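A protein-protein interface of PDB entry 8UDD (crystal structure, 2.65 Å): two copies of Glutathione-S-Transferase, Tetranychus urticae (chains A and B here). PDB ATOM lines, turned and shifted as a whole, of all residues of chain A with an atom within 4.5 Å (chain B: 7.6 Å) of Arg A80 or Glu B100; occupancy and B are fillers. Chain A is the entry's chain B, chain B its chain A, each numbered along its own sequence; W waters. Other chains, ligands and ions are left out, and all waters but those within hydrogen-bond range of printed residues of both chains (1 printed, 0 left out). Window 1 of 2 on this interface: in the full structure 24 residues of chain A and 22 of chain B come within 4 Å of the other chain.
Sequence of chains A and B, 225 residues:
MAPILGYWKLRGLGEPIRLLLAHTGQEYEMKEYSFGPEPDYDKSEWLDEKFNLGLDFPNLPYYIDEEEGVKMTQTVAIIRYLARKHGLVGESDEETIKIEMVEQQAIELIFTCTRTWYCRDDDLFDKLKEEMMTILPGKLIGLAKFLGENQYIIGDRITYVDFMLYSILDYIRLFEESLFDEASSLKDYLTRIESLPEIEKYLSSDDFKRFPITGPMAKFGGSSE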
ATOM      1  N   VAL A  76      16.891 -13.562  16.143  1.00  0.00           N
ATOM      2  CA  VAL A  76      16.851 -12.280  15.385  1.00  0.00           C
ATOM      3  C   VAL A  76      16.733 -11.118  16.368  1.00  0.00           C
ATOM      4  O   VAL A  76      17.364 -10.090  16.149  1.00  0.00           O
ATOM      5  CB  VAL A  76      15.701 -12.287  14.369  1.00  0.00           C
ATOM      6  CG1 VAL A  76      15.535 -10.953  13.666  1.00  0.00           C
ATOM      7  CG2 VAL A  76      15.866 -13.413  13.369  1.00  0.00           C
ATOM      8  N   ALA A  77      15.956 -11.302  17.425  1.00  0.00           N
ATOM      9  CA  ALA A  77      15.773 -10.240  18.429  1.00  0.00           C
ATOM     10  C   ALA A  77      17.061 -10.073  19.226  1.00  0.00           C
ATOM     11  O   ALA A  77      17.401  -8.933  19.553  1.00  0.00           O
ATOM     12  CB  ALA A  77      14.625 -10.598  19.325  1.00  0.00           C
ATOM     13  N   ILE A  78      17.737 -11.179  19.529  1.00  0.00           N
ATOM     14  CA  ILE A  78      19.007 -11.065  20.247  1.00  0.00           C
ATOM     15  C   ILE A  78      20.056 -10.328  19.395  1.00  0.00           C
ATOM     16  O   ILE A  78      20.699  -9.400  19.858  1.00  0.00           O
ATOM     17  CB  ILE A  78      19.511 -12.437  20.722  1.00  0.00           C
ATOM     18  CG1 ILE A  78      18.541 -13.079  21.726  1.00  0.00           C
ATOM     19  CG2 ILE A  78      20.915 -12.314  21.287  1.00  0.00           C
ATOM     20  CD1 ILE A  78      18.927 -14.491  22.133  1.00  0.00           C
ATOM     21  N   ILE A  79      20.198 -10.703  18.127  1.00  0.00           N
ATOM     22  CA  ILE A  79      21.239 -10.107  17.311  1.00  0.00           C
ATOM     23  C   ILE A  79      20.858  -8.666  16.950  1.00  0.00           C
ATOM     24  O   ILE A  79      21.728  -7.792  16.846  1.00  0.00           O
ATOM     25  CB  ILE A  79      21.561 -11.022  16.109  1.00  0.00           C
ATOM     26  CG1 ILE A  79      22.906 -10.657  15.482  1.00  0.00           C
ATOM     27  CG2 ILE A  79      20.438 -11.036  15.076  1.00  0.00           C
ATOM     28  CD1 ILE A  79      23.332 -11.593  14.367  1.00  0.00           C
ATOM     29  N   ARG A  80      19.560  -8.356  16.830  1.00  0.00           N
ATOM     30  CA  ARG A  80      19.184  -6.966  16.579  1.00  0.00           C
ATOM     31  C   ARG A  80      19.539  -6.105  17.788  1.00  0.00           C
ATOM     32  O   ARG A  80      19.956  -4.946  17.626  1.00  0.00           O
ATOM     33  CB  ARG A  80      17.718  -6.845  16.170  1.00  0.00           C
ATOM     34  CG  ARG A  80      17.479  -7.417  14.780  1.00  0.00           C
ATOM     35  CD  ARG A  80      16.058  -7.375  14.277  1.00  0.00           C
ATOM     36  NE  ARG A  80      15.461  -6.057  14.412  1.00  0.00           N
ATOM     37  CZ  ARG A  80      15.299  -5.175  13.427  1.00  0.00           C
ATOM     38  NH1 ARG A  80      16.186  -5.121  12.438  1.00  0.00           N
ATOM     39  NH2 ARG A  80      14.298  -4.294  13.507  1.00  0.00           N
ATOM     40  N   TYR A  81      19.406  -6.690  18.994  1.00  0.00           N
ATOM     41  CA  TYR A  81      19.664  -5.955  20.233  1.00  0.00           C
ATOM     42  C   TYR A  81      21.151  -5.585  20.331  1.00  0.00           C
ATOM     43  O   TYR A  81      21.509  -4.432  20.620  1.00  0.00           O
ATOM     44  CB  TYR A  81      19.201  -6.774  21.437  1.00  0.00           C
ATOM     45  CG  TYR A  81      19.842  -6.350  22.732  1.00  0.00           C
ATOM     46  CD1 TYR A  81      19.423  -5.211  23.399  1.00  0.00           C
ATOM     47  CD2 TYR A  81      20.926  -7.044  23.244  1.00  0.00           C
ATOM     48  CE1 TYR A  81      20.012  -4.816  24.588  1.00  0.00           C
ATOM     49  CE2 TYR A  81      21.561  -6.633  24.408  1.00  0.00           C
ATOM     50  CZ  TYR A  81      21.111  -5.512  25.080  1.00  0.00           C
ATOM     51  OH  TYR A  81      21.789  -5.095  26.223  1.00  0.00           O
ATOM     52  N   LEU A  82      22.011  -6.573  20.089  1.00  0.00           N
ATOM     53  CA  LEU A  82      23.476  -6.349  20.182  1.00  0.00           C
ATOM     54  C   LEU A  82      23.926  -5.420  19.050  1.00  0.00           C
ATOM     55  O   LEU A  82      24.830  -4.605  19.284  1.00  0.00           O
ATOM     56  CB  LEU A  82      24.161  -7.714  20.102  1.00  0.00           C
ATOM     57  CG  LEU A  82      23.889  -8.654  21.273  1.00  0.00           C
ATOM     58  CD1 LEU A  82      24.466 -10.033  21.003  1.00  0.00           C
ATOM     59  CD2 LEU A  82      24.461  -8.083  22.559  1.00  0.00           C
ATOM     60  N   ALA A  83      23.297  -5.527  17.879  1.00  0.00           N
ATOM     61  CA  ALA A  83      23.657  -4.669  16.728  1.00  0.00           C
ATOM     62  C   ALA A  83      23.412  -3.197  17.071  1.00  0.00           C
ATOM     63  O   ALA A  83      24.290  -2.369  16.780  1.00  0.00           O
ATOM     64  CB  ALA A  83      22.854  -5.087  15.529  1.00  0.00           C
ATOM     65  N   ARG A  84      22.260  -2.886  17.664  1.00  0.00           N
ATOM     66  CA  ARG A  84      21.915  -1.485  18.016  1.00  0.00           C
ATOM     67  C   ARG A  84      22.837  -1.010  19.138  1.00  0.00           C
ATOM     68  O   ARG A  84      23.094   0.202  19.217  1.00  0.00           O
ATOM     69  CB  ARG A  84      20.445  -1.398  18.434  1.00  0.00           C
ATOM     70  CG  ARG A  84      19.455  -1.746  17.333  1.00  0.00           C
ATOM     71  CD  ARG A  84      18.025  -1.678  17.830  1.00  0.00           C
ATOM     72  NE  ARG A  84      17.819  -2.479  19.028  1.00  0.00           N
ATOM     73  CZ  ARG A  84      17.021  -3.536  19.090  1.00  0.00           C
ATOM     74  NH1 ARG A  84      16.706  -4.062  20.260  1.00  0.00           N
ATOM     75  NH2 ARG A  84      16.542  -4.065  17.979  1.00  0.00           N
ATOM     76  N   GLU A 100      16.970  -5.444   6.420  1.00  0.00           N
ATOM     77  CA  GLU A 100      15.893  -6.275   6.940  1.00  0.00           C
ATOM     78  C   GLU A 100      15.381  -7.225   5.855  1.00  0.00           C
ATOM     79  O   GLU A 100      14.953  -8.333   6.162  1.00  0.00           O
ATOM     80  CB  GLU A 100      14.785  -5.389   7.514  1.00  0.00           C
ATOM     81  CG  GLU A 100      15.196  -4.713   8.812  1.00  0.00           C
ATOM     82  CD  GLU A 100      14.161  -3.829   9.500  1.00  0.00           C
ATOM     83  OE1 GLU A 100      13.128  -3.427   8.847  1.00  0.00           O
ATOM     84  OE2 GLU A 100      14.375  -3.520  10.699  1.00  0.00           O
ATOM     85  N   GLU A 103      18.096  -9.793   6.054  1.00  0.00           N
ATOM     86  CA  GLU A 103      17.885 -10.568   7.263  1.00  0.00           C
ATOM     87  C   GLU A 103      16.882 -11.689   6.998  1.00  0.00           C
ATOM     88  O   GLU A 103      17.120 -12.843   7.369  1.00  0.00           O
ATOM     89  CB  GLU A 103      17.344  -9.674   8.359  1.00  0.00           C
ATOM     90  CG  GLU A 103      16.935 -10.402   9.635  1.00  0.00           C
ATOM     91  CD  GLU A 103      16.114  -9.474  10.525  1.00  0.00           C
ATOM     92  OE1 GLU A 103      16.717  -8.466  11.004  1.00  0.00           O
ATOM     93  OE2 GLU A 103      14.848  -9.709  10.660  1.00  0.00           O
ATOM     94  N   TYR A 160      24.941  -6.364  11.135  1.00  0.00           N
ATOM     95  CA  TYR A 160      24.669  -7.641  11.781  1.00  0.00           C
ATOM     96  C   TYR A 160      24.279  -8.721  10.774  1.00  0.00           C
ATOM     97  O   TYR A 160      24.458  -9.915  11.007  1.00  0.00           O
ATOM     98  CB  TYR A 160      23.575  -7.499  12.844  1.00  0.00           C
ATOM     99  CG  TYR A 160      22.178  -7.224  12.335  1.00  0.00           C
ATOM    100  CD1 TYR A 160      21.288  -8.267  12.107  1.00  0.00           C
ATOM    101  CD2 TYR A 160      21.684  -5.933  12.214  1.00  0.00           C
ATOM    102  CE1 TYR A 160      19.985  -8.044  11.693  1.00  0.00           C
ATOM    103  CE2 TYR A 160      20.389  -5.691  11.789  1.00  0.00           C
ATOM    104  CZ  TYR A 160      19.528  -6.748  11.542  1.00  0.00           C
ATOM    105  OH  TYR A 160      18.222  -6.546  11.119  1.00  0.00           O
ATOM    106  N   VAL B  76       8.148  -9.534   7.052  1.00  0.00           N
ATOM    107  CA  VAL B  76       8.613  -8.905   8.323  1.00  0.00           C
ATOM    108  C   VAL B  76       9.213  -7.534   8.011  1.00  0.00           C
ATOM    109  O   VAL B  76       8.937  -6.588   8.763  1.00  0.00           O
ATOM    110  CB  VAL B  76       9.619  -9.818   9.043  1.00  0.00           C
ATOM    111  CG1 VAL B  76       9.983  -9.286  10.419  1.00  0.00           C
ATOM    112  CG2 VAL B  76       9.094 -11.239   9.139  1.00  0.00           C
ATOM    113  N   ARG B  80       7.672  -3.982   9.265  1.00  0.00           N
ATOM    114  CA  ARG B  80       8.494  -3.119  10.097  1.00  0.00           C
ATOM    115  C   ARG B  80       8.594  -1.724   9.470  1.00  0.00           C
ATOM    116  O   ARG B  80       8.598  -0.713  10.186  1.00  0.00           O
ATOM    117  CB  ARG B  80       9.884  -3.712  10.340  1.00  0.00           C
ATOM    118  CG  ARG B  80       9.951  -4.944  11.238  1.00  0.00           C
ATOM    119  CD  ARG B  80      11.394  -5.006  11.761  1.00  0.00           C
ATOM    120  NE  ARG B  80      11.861  -6.302  12.226  1.00  0.00           N
ATOM    121  CZ  ARG B  80      12.570  -7.162  11.491  1.00  0.00           C
ATOM    122  NH1 ARG B  80      12.694  -6.975  10.184  1.00  0.00           N
ATOM    123  NH2 ARG B  80      13.128  -8.223  12.059  1.00  0.00           N
ATOM    124  N   ARG B  84       7.336   1.692  11.307  1.00  0.00           N
ATOM    125  CA  ARG B  84       8.205   2.831  11.597  1.00  0.00           C
ATOM    126  C   ARG B  84       7.582   4.100  11.042  1.00  0.00           C
ATOM    127  O   ARG B  84       7.604   5.142  11.684  1.00  0.00           O
ATOM    128  CB  ARG B  84       9.596   2.635  11.001  1.00  0.00           C
ATOM    129  CG  ARG B  84      10.414   1.568  11.714  1.00  0.00           C
ATOM    130  CD  ARG B  84      11.846   1.530  11.237  1.00  0.00           C
ATOM    131  NE  ARG B  84      11.894   1.335   9.791  1.00  0.00           N
ATOM    132  CZ  ARG B  84      12.134   0.183   9.166  1.00  0.00           C
ATOM    133  NH1 ARG B  84      12.274   0.136   7.845  1.00  0.00           N
ATOM    134  NH2 ARG B  84      12.251  -0.925   9.871  1.00  0.00           N
ATOM    135  N   GLY B  90       8.515   0.279  18.782  1.00  0.00           N
ATOM    136  CA  GLY B  90       8.941   0.577  20.160  1.00  0.00           C
ATOM    137  C   GLY B  90       9.458   1.993  20.296  1.00  0.00           C
ATOM    138  O   GLY B  90      10.081   2.486  19.344  1.00  0.00           O
ATOM    139  N   ASP B  93      14.214   0.932  24.108  1.00  0.00           N
ATOM    140  CA  ASP B  93      14.850  -0.386  23.865  1.00  0.00           C
ATOM    141  C   ASP B  93      14.088  -1.432  24.682  1.00  0.00           C
ATOM    142  O   ASP B  93      13.909  -2.547  24.173  1.00  0.00           O
ATOM    143  CB  ASP B  93      16.349  -0.364  24.167  1.00  0.00           C
ATOM    144  CG  ASP B  93      17.089  -1.575  23.626  1.00  0.00           C
ATOM    145  OD1 ASP B  93      17.004  -1.814  22.408  1.00  0.00           O
ATOM    146  OD2 ASP B  93      17.755  -2.256  24.425  1.00  0.00           O
ATOM    147  N   GLU B  94      13.622  -1.075  25.883  1.00  0.00           N
ATOM    148  CA  GLU B  94      12.829  -2.050  26.627  1.00  0.00           C
ATOM    149  C   GLU B  94      11.670  -2.515  25.750  1.00  0.00           C
ATOM    150  O   GLU B  94      11.503  -3.718  25.604  1.00  0.00           O
ATOM    151  CB  GLU B  94      12.308  -1.544  27.977  1.00  0.00           C
ATOM    152  CG  GLU B  94      13.353  -1.510  29.085  1.00  0.00           C
ATOM    153  CD  GLU B  94      14.659  -0.834  28.665  1.00  0.00           C
ATOM    154  OE1 GLU B  94      14.648   0.435  28.383  1.00  0.00           O
ATOM    155  OE2 GLU B  94      15.690  -1.580  28.557  1.00  0.00           O
ATOM    156  N   GLU B  95      10.919  -1.583  25.130  1.00  0.00           N
ATOM    157  CA  GLU B  95       9.773  -1.962  24.323  1.00  0.00           C
ATOM    158  C   GLU B  95      10.206  -2.707  23.070  1.00  0.00           C
ATOM    159  O   GLU B  95       9.542  -3.661  22.648  1.00  0.00           O
ATOM    160  CB  GLU B  95       8.942  -0.775  23.864  1.00  0.00           C
ATOM    161  CG  GLU B  95       8.268  -0.029  24.974  1.00  0.00           C
ATOM    162  CD  GLU B  95       7.413   1.153  24.554  1.00  0.00           C
ATOM    163  OE1 GLU B  95       7.357   1.478  23.320  1.00  0.00           O
ATOM    164  OE2 GLU B  95       6.818   1.755  25.482  1.00  0.00           O
ATOM    165  N   THR B  96      11.292  -2.261  22.455  1.00  0.00           N
ATOM    166  CA  THR B  96      11.724  -2.845  21.189  1.00  0.00           C
ATOM    167  C   THR B  96      12.101  -4.321  21.356  1.00  0.00           C
ATOM    168  O   THR B  96      11.780  -5.136  20.483  1.00  0.00           O
ATOM    169  CB  THR B  96      12.918  -2.064  20.621  1.00  0.00           C
ATOM    170  OG1 THR B  96      12.440  -0.768  20.219  1.00  0.00           O
ATOM    171  CG2 THR B  96      13.582  -2.832  19.494  1.00  0.00           C
ATOM    172  N   ILE B  97      12.790  -4.639  22.467  1.00  0.00           N
ATOM    173  CA  ILE B  97      13.139  -6.005  22.840  1.00  0.00           C
ATOM    174  C   ILE B  97      11.867  -6.857  22.940  1.00  0.00           C
ATOM    175  O   ILE B  97      11.768  -7.899  22.299  1.00  0.00           O
ATOM    176  CB  ILE B  97      13.944  -5.997  24.166  1.00  0.00           C
ATOM    177  CG1 ILE B  97      15.352  -5.411  24.002  1.00  0.00           C
ATOM    178  CG2 ILE B  97      13.990  -7.371  24.835  1.00  0.00           C
ATOM    179  CD1 ILE B  97      16.033  -5.082  25.333  1.00  0.00           C
ATOM    180  N   LYS B  98      10.896  -6.413  23.748  1.00  0.00           N
ATOM    181  CA  LYS B  98       9.621  -7.095  23.904  1.00  0.00           C
ATOM    182  C   LYS B  98       8.906  -7.287  22.564  1.00  0.00           C
ATOM    183  O   LYS B  98       8.434  -8.392  22.264  1.00  0.00           O
ATOM    184  CB  LYS B  98       8.691  -6.284  24.805  1.00  0.00           C
ATOM    185  CG  LYS B  98       9.027  -6.163  26.296  1.00  0.00           C
ATOM    186  CD  LYS B  98       7.786  -5.597  27.020  1.00  0.00           C
ATOM    187  CE  LYS B  98       8.009  -4.554  28.089  1.00  0.00           C
ATOM    188  NZ  LYS B  98       8.780  -5.106  29.228  1.00  0.00           N
ATOM    189  N   ILE B  99       8.807  -6.221  21.762  1.00  0.00           N
ATOM    190  CA  ILE B  99       8.121  -6.302  20.470  1.00  0.00           C
ATOM    191  C   ILE B  99       8.798  -7.317  19.543  1.00  0.00           C
ATOM    192  O   ILE B  99       8.133  -8.057  18.819  1.00  0.00           O
ATOM    193  CB  ILE B  99       8.051  -4.908  19.813  1.00  0.00           C
ATOM    194  CG1 ILE B  99       7.073  -4.007  20.575  1.00  0.00           C
ATOM    195  CG2 ILE B  99       7.744  -4.958  18.319  1.00  0.00           C
ATOM    196  CD1 ILE B  99       7.118  -2.534  20.159  1.00  0.00           C
ATOM    197  N   GLU B 100      10.122  -7.312  19.498  1.00  0.00           N
ATOM    198  CA  GLU B 100      10.835  -8.135  18.532  1.00  0.00           C
ATOM    199  C   GLU B 100      10.854  -9.598  18.990  1.00  0.00           C
ATOM    200  O   GLU B 100      10.829 -10.499  18.148  1.00  0.00           O
ATOM    201  CB  GLU B 100      12.256  -7.603  18.317  1.00  0.00           C
ATOM    202  CG  GLU B 100      12.273  -6.299  17.551  1.00  0.00           C
ATOM    203  CD  GLU B 100      13.611  -5.615  17.329  1.00  0.00           C
ATOM    204  OE1 GLU B 100      14.676  -6.015  17.976  1.00  0.00           O
ATOM    205  OE2 GLU B 100      13.571  -4.618  16.562  1.00  0.00           O
ATOM    206  N   MET B 101      10.862  -9.849  20.308  1.00  0.00           N
ATOM    207  CA  MET B 101      10.715 -11.224  20.765  1.00  0.00           C
ATOM    208  C   MET B 101       9.349 -11.787  20.352  1.00  0.00           C
ATOM    209  O   MET B 101       9.269 -12.909  19.865  1.00  0.00           O
ATOM    210  CB  MET B 101      10.880 -11.317  22.280  1.00  0.00           C
ATOM    211  CG  MET B 101      12.277 -11.123  22.704  1.00  0.00           C
ATOM    212  SD  MET B 101      12.574 -11.928  24.260  1.00  0.00           S
ATOM    213  CE  MET B 101      11.868 -10.732  25.404  1.00  0.00           C
ATOM    214  N   VAL B 102       8.285 -11.000  20.529  1.00  0.00           N
ATOM    215  CA  VAL B 102       6.915 -11.374  20.172  1.00  0.00           C
ATOM    216  C   VAL B 102       6.765 -11.494  18.657  1.00  0.00           C
ATOM    217  O   VAL B 102       6.029 -12.351  18.153  1.00  0.00           O
ATOM    218  CB  VAL B 102       5.906 -10.322  20.700  1.00  0.00           C
ATOM    219  CG1 VAL B 102       4.516 -10.589  20.181  1.00  0.00           C
ATOM    220  CG2 VAL B 102       5.898 -10.220  22.216  1.00  0.00           C
ATOM    221  N   GLU B 103       7.407 -10.583  17.928  1.00  0.00           N
ATOM    222  CA  GLU B 103       7.430 -10.700  16.477  1.00  0.00           C
ATOM    223  C   GLU B 103       7.927 -12.083  16.085  1.00  0.00           C
ATOM    224  O   GLU B 103       7.336 -12.734  15.232  1.00  0.00           O
ATOM    225  CB  GLU B 103       8.323  -9.631  15.859  1.00  0.00           C
ATOM    226  CG  GLU B 103       8.522  -9.779  14.370  1.00  0.00           C
ATOM    227  CD  GLU B 103       9.720  -8.971  13.916  1.00  0.00           C
ATOM    228  OE1 GLU B 103      10.749  -9.606  13.629  1.00  0.00           O
ATOM    229  OE2 GLU B 103       9.650  -7.715  13.986  1.00  0.00           O
ATOM    230  N   GLN B 104       9.014 -12.512  16.720  1.00  0.00           N
ATOM    231  CA  GLN B 104       9.707 -13.736  16.325  1.00  0.00           C
ATOM    232  C   GLN B 104       8.964 -14.926  16.885  1.00  0.00           C
ATOM    233  O   GLN B 104       8.837 -15.941  16.230  1.00  0.00           O
ATOM    234  CB  GLN B 104      11.167 -13.724  16.812  1.00  0.00           C
ATOM    235  CG  GLN B 104      12.016 -12.686  16.107  1.00  0.00           C
ATOM    236  CD  GLN B 104      12.071 -13.056  14.660  1.00  0.00           C
ATOM    237  OE1 GLN B 104      12.480 -14.172  14.330  1.00  0.00           O
ATOM    238  NE2 GLN B 104      11.651 -12.136  13.802  1.00  0.00           N
ATOM    239  N   GLN B 105       8.417 -14.781  18.088  1.00  0.00           N
ATOM    240  CA  GLN B 105       7.563 -15.834  18.624  1.00  0.00           C
ATOM    241  C   GLN B 105       6.355 -16.026  17.703  1.00  0.00           C
ATOM    242  O   GLN B 105       6.000 -17.153  17.427  1.00  0.00           O
ATOM    243  CB  GLN B 105       7.220 -15.517  20.073  1.00  0.00           C
ATOM    244  CG  GLN B 105       6.328 -16.547  20.715  1.00  0.00           C
ATOM    245  CD  GLN B 105       6.911 -17.925  20.896  1.00  0.00           C
ATOM    246  OE1 GLN B 105       7.010 -18.701  19.951  1.00  0.00           O
ATOM    247  NE2 GLN B 105       7.121 -18.310  22.142  1.00  0.00           N
ATOM    248  N   ALA B 106       5.787 -14.945  17.152  1.00  0.00           N
ATOM    249  CA  ALA B 106       4.678 -15.062  16.207  1.00  0.00           C
ATOM    250  C   ALA B 106       5.088 -15.856  14.960  1.00  0.00           C
ATOM    251  O   ALA B 106       4.405 -16.801  14.597  1.00  0.00           O
ATOM    252  CB  ALA B 106       4.127 -13.685  15.837  1.00  0.00           C
ATOM    253  N   ILE B 107       6.196 -15.471  14.313  1.00  0.00           N
ATOM    254  CA  ILE B 107       6.686 -16.114  13.095  1.00  0.00           C
ATOM    255  C   ILE B 107       7.059 -17.576  13.326  1.00  0.00           C
ATOM    256  O   ILE B 107       6.914 -18.398  12.430  1.00  0.00           O
ATOM    257  CB  ILE B 107       7.883 -15.310  12.562  1.00  0.00           C
ATOM    258  CG1 ILE B 107       7.403 -14.073  11.826  1.00  0.00           C
ATOM    259  CG2 ILE B 107       8.797 -16.122  11.680  1.00  0.00           C
ATOM    260  CD1 ILE B 107       8.424 -12.991  11.902  1.00  0.00           C
ATOM    261  N   ILE B 154       2.124  -4.862  24.355  1.00  0.00           N
ATOM    262  CA  ILE B 154       3.132  -4.008  24.995  1.00  0.00           C
ATOM    263  C   ILE B 154       2.486  -3.067  26.013  1.00  0.00           C
ATOM    264  O   ILE B 154       3.174  -2.235  26.573  1.00  0.00           O
ATOM    265  CB  ILE B 154       3.884  -3.226  23.891  1.00  0.00           C
ATOM    266  CG1 ILE B 154       4.514  -4.177  22.878  1.00  0.00           C
ATOM    267  CG2 ILE B 154       4.916  -2.233  24.382  1.00  0.00           C
ATOM    268  CD1 ILE B 154       5.503  -5.158  23.467  1.00  0.00           C
ATOM    269  N   TYR B 160       2.888  -3.014  15.780  1.00  0.00           N
ATOM    270  CA  TYR B 160       2.653  -3.801  14.572  1.00  0.00           C
ATOM    271  C   TYR B 160       2.484  -5.281  14.884  1.00  0.00           C
ATOM    272  O   TYR B 160       1.853  -6.046  14.148  1.00  0.00           O
ATOM    273  CB  TYR B 160       3.812  -3.639  13.587  1.00  0.00           C
ATOM    274  CG  TYR B 160       5.154  -4.190  14.003  1.00  0.00           C
ATOM    275  CD1 TYR B 160       5.564  -5.449  13.603  1.00  0.00           C
ATOM    276  CD2 TYR B 160       6.099  -3.379  14.626  1.00  0.00           C
ATOM    277  CE1 TYR B 160       6.834  -5.922  13.893  1.00  0.00           C
ATOM    278  CE2 TYR B 160       7.358  -3.843  14.962  1.00  0.00           C
ATOM    279  CZ  TYR B 160       7.747  -5.109  14.549  1.00  0.00           C
ATOM    280  OH  TYR B 160       9.014  -5.569  14.852  1.00  0.00           O
ATOM    281  N   VAL B 161       3.028  -5.673  16.024  1.00  0.00           N
ATOM    282  CA  VAL B 161       3.168  -7.077  16.369  1.00  0.00           C
ATOM    283  C   VAL B 161       1.815  -7.602  16.861  1.00  0.00           C
ATOM    284  O   VAL B 161       1.577  -8.797  16.831  1.00  0.00           O
ATOM    285  CB  VAL B 161       4.358  -7.184  17.350  1.00  0.00           C
ATOM    286  CG1 VAL B 161       4.154  -6.449  18.661  1.00  0.00           C
ATOM    287  CG2 VAL B 161       4.745  -8.600  17.581  1.00  0.00           C
HETATM  288  O   HOH W   1      20.003  -2.078  22.175  1.00  0.00           O
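The guanidinium group (NE) of Arg B80 is in salt-bridge range of the side-chain carboxylate (OE2) of Glu B103, 3.2 Å away.
The side-chain amide nitrogen of Gln B104 lies within hydrogen-bond range of the side-chain carboxylate of Glu B103, 2.7 Å away.
The side-chain carboxylate (OE2) of Glu A100 lies within salt-bridge range of the guanidinium group (NH2) of Arg A80.
The side-chain carboxylate (OE1) of Glu A103 is in salt-bridge range of the guanidinium group (NH1) of Arg A80 (3.7 Å).
The side-chain hydroxyl of Tyr A160 is in hydrogen-bond range of the guanidinium group of Arg A80, at 2.8 Å.
The side-chain carboxylate (OE1) of Glu A103 is in hydrogen-bond range of the side-chain hydroxyl (OH) of Tyr A160, at 2.4 Å.
Arg A80 touches its own counterpart, Arg B80.
Arg A80 touches Glu B100, and with the chains exchanged Glu A100 touches Arg B80.
Arg A84 touches Glu B100, and with the chains exchanged Glu A100 touches Arg B84.
Glu A103 touches Arg B80, but with the chains exchanged Arg A80 does not touch Glu B103 (5.8 Å).
Positions printed for both chains: 76, 80, 84, 100, 103 and 160.
Of the 14 pairs that touch across the chains among the printed residues, 5 have their exchanged pair printed and touching as well.
Printed residues of chain B within 4 Å of Val A76: Arg B80 (3.98 Å) and Gln B104 (3.6 Å).
Of the printed residues of chain B, Ala A77 touches Glu B100 (3.9 Å) and Met B101 (3.96 Å).
Arg A80 touches just these residues of chain B: Arg B80 (3.4 Å) and Glu B100 (3.2 Å).
Val B76 touches none of the printed residues of chain A.
Printed residues of chain A within 4 Å of Gln B104: Val A76.
The nearest printed residue of chain A that does not touch Glu B100 is Tyr A81 (4.9 Å).
The nearest printed residue of chain A that does not touch Arg B80 is Tyr A160 (5.4 Å).
Of the 12 printed residues of chain A, 7 touch a printed residue of chain B.
Hydrophobic or aromatic side chains of chain B within 4 Å of the printed part of chain A: Ile B97.
The side-chain carboxylate (OE1) of Glu A100 lies within salt-bridge range of the guanidinium group (NH1) of Arg B80 (3.8 Å).
OE2 of Glu A103 is in salt-bridge range of NH2 of Arg B80 (2.7 Å).
The guanidinium group (NH2) of Arg B84 lies within salt-bridge range of the side-chain carboxylate (OE1) of Glu A100, 2.8 Å away.
OD1 of Asp B93 is in salt-bridge range of NH1 of Arg A84 (3.1 Å).
The side-chain carboxylate (OE2) of Glu B100 is in salt-bridge range of the guanidinium group (NH2) of Arg A80 (3.2 Å).
The guanidinium group of Arg A84 lies within salt-bridge range of the side-chain carboxylate of Glu B100 (2.7 Å).
The guanidinium group of Arg A80 sits close to the guanidinium group of Arg B80 (3.4 Å).
Val A76 touches Arg B80.
Val A76 touches Gln B104.
Ala A77 touches Glu B100.
Met B101 touches Ala A77.
CE1 of Tyr A81 touches OD2 of Asp B93, 3.4 Å away.
Ile B97 touches Tyr A81 (CD1 to CD1, 3.9 Å).
Arg A84 touches Thr B96.
Water W1 lies within hydrogen-bond range of the side-chain carboxylate (OD1) of Asp B93 (3.0 Å) and the backbone carbonyl oxygen (O) of Tyr A81 (3.2 Å).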
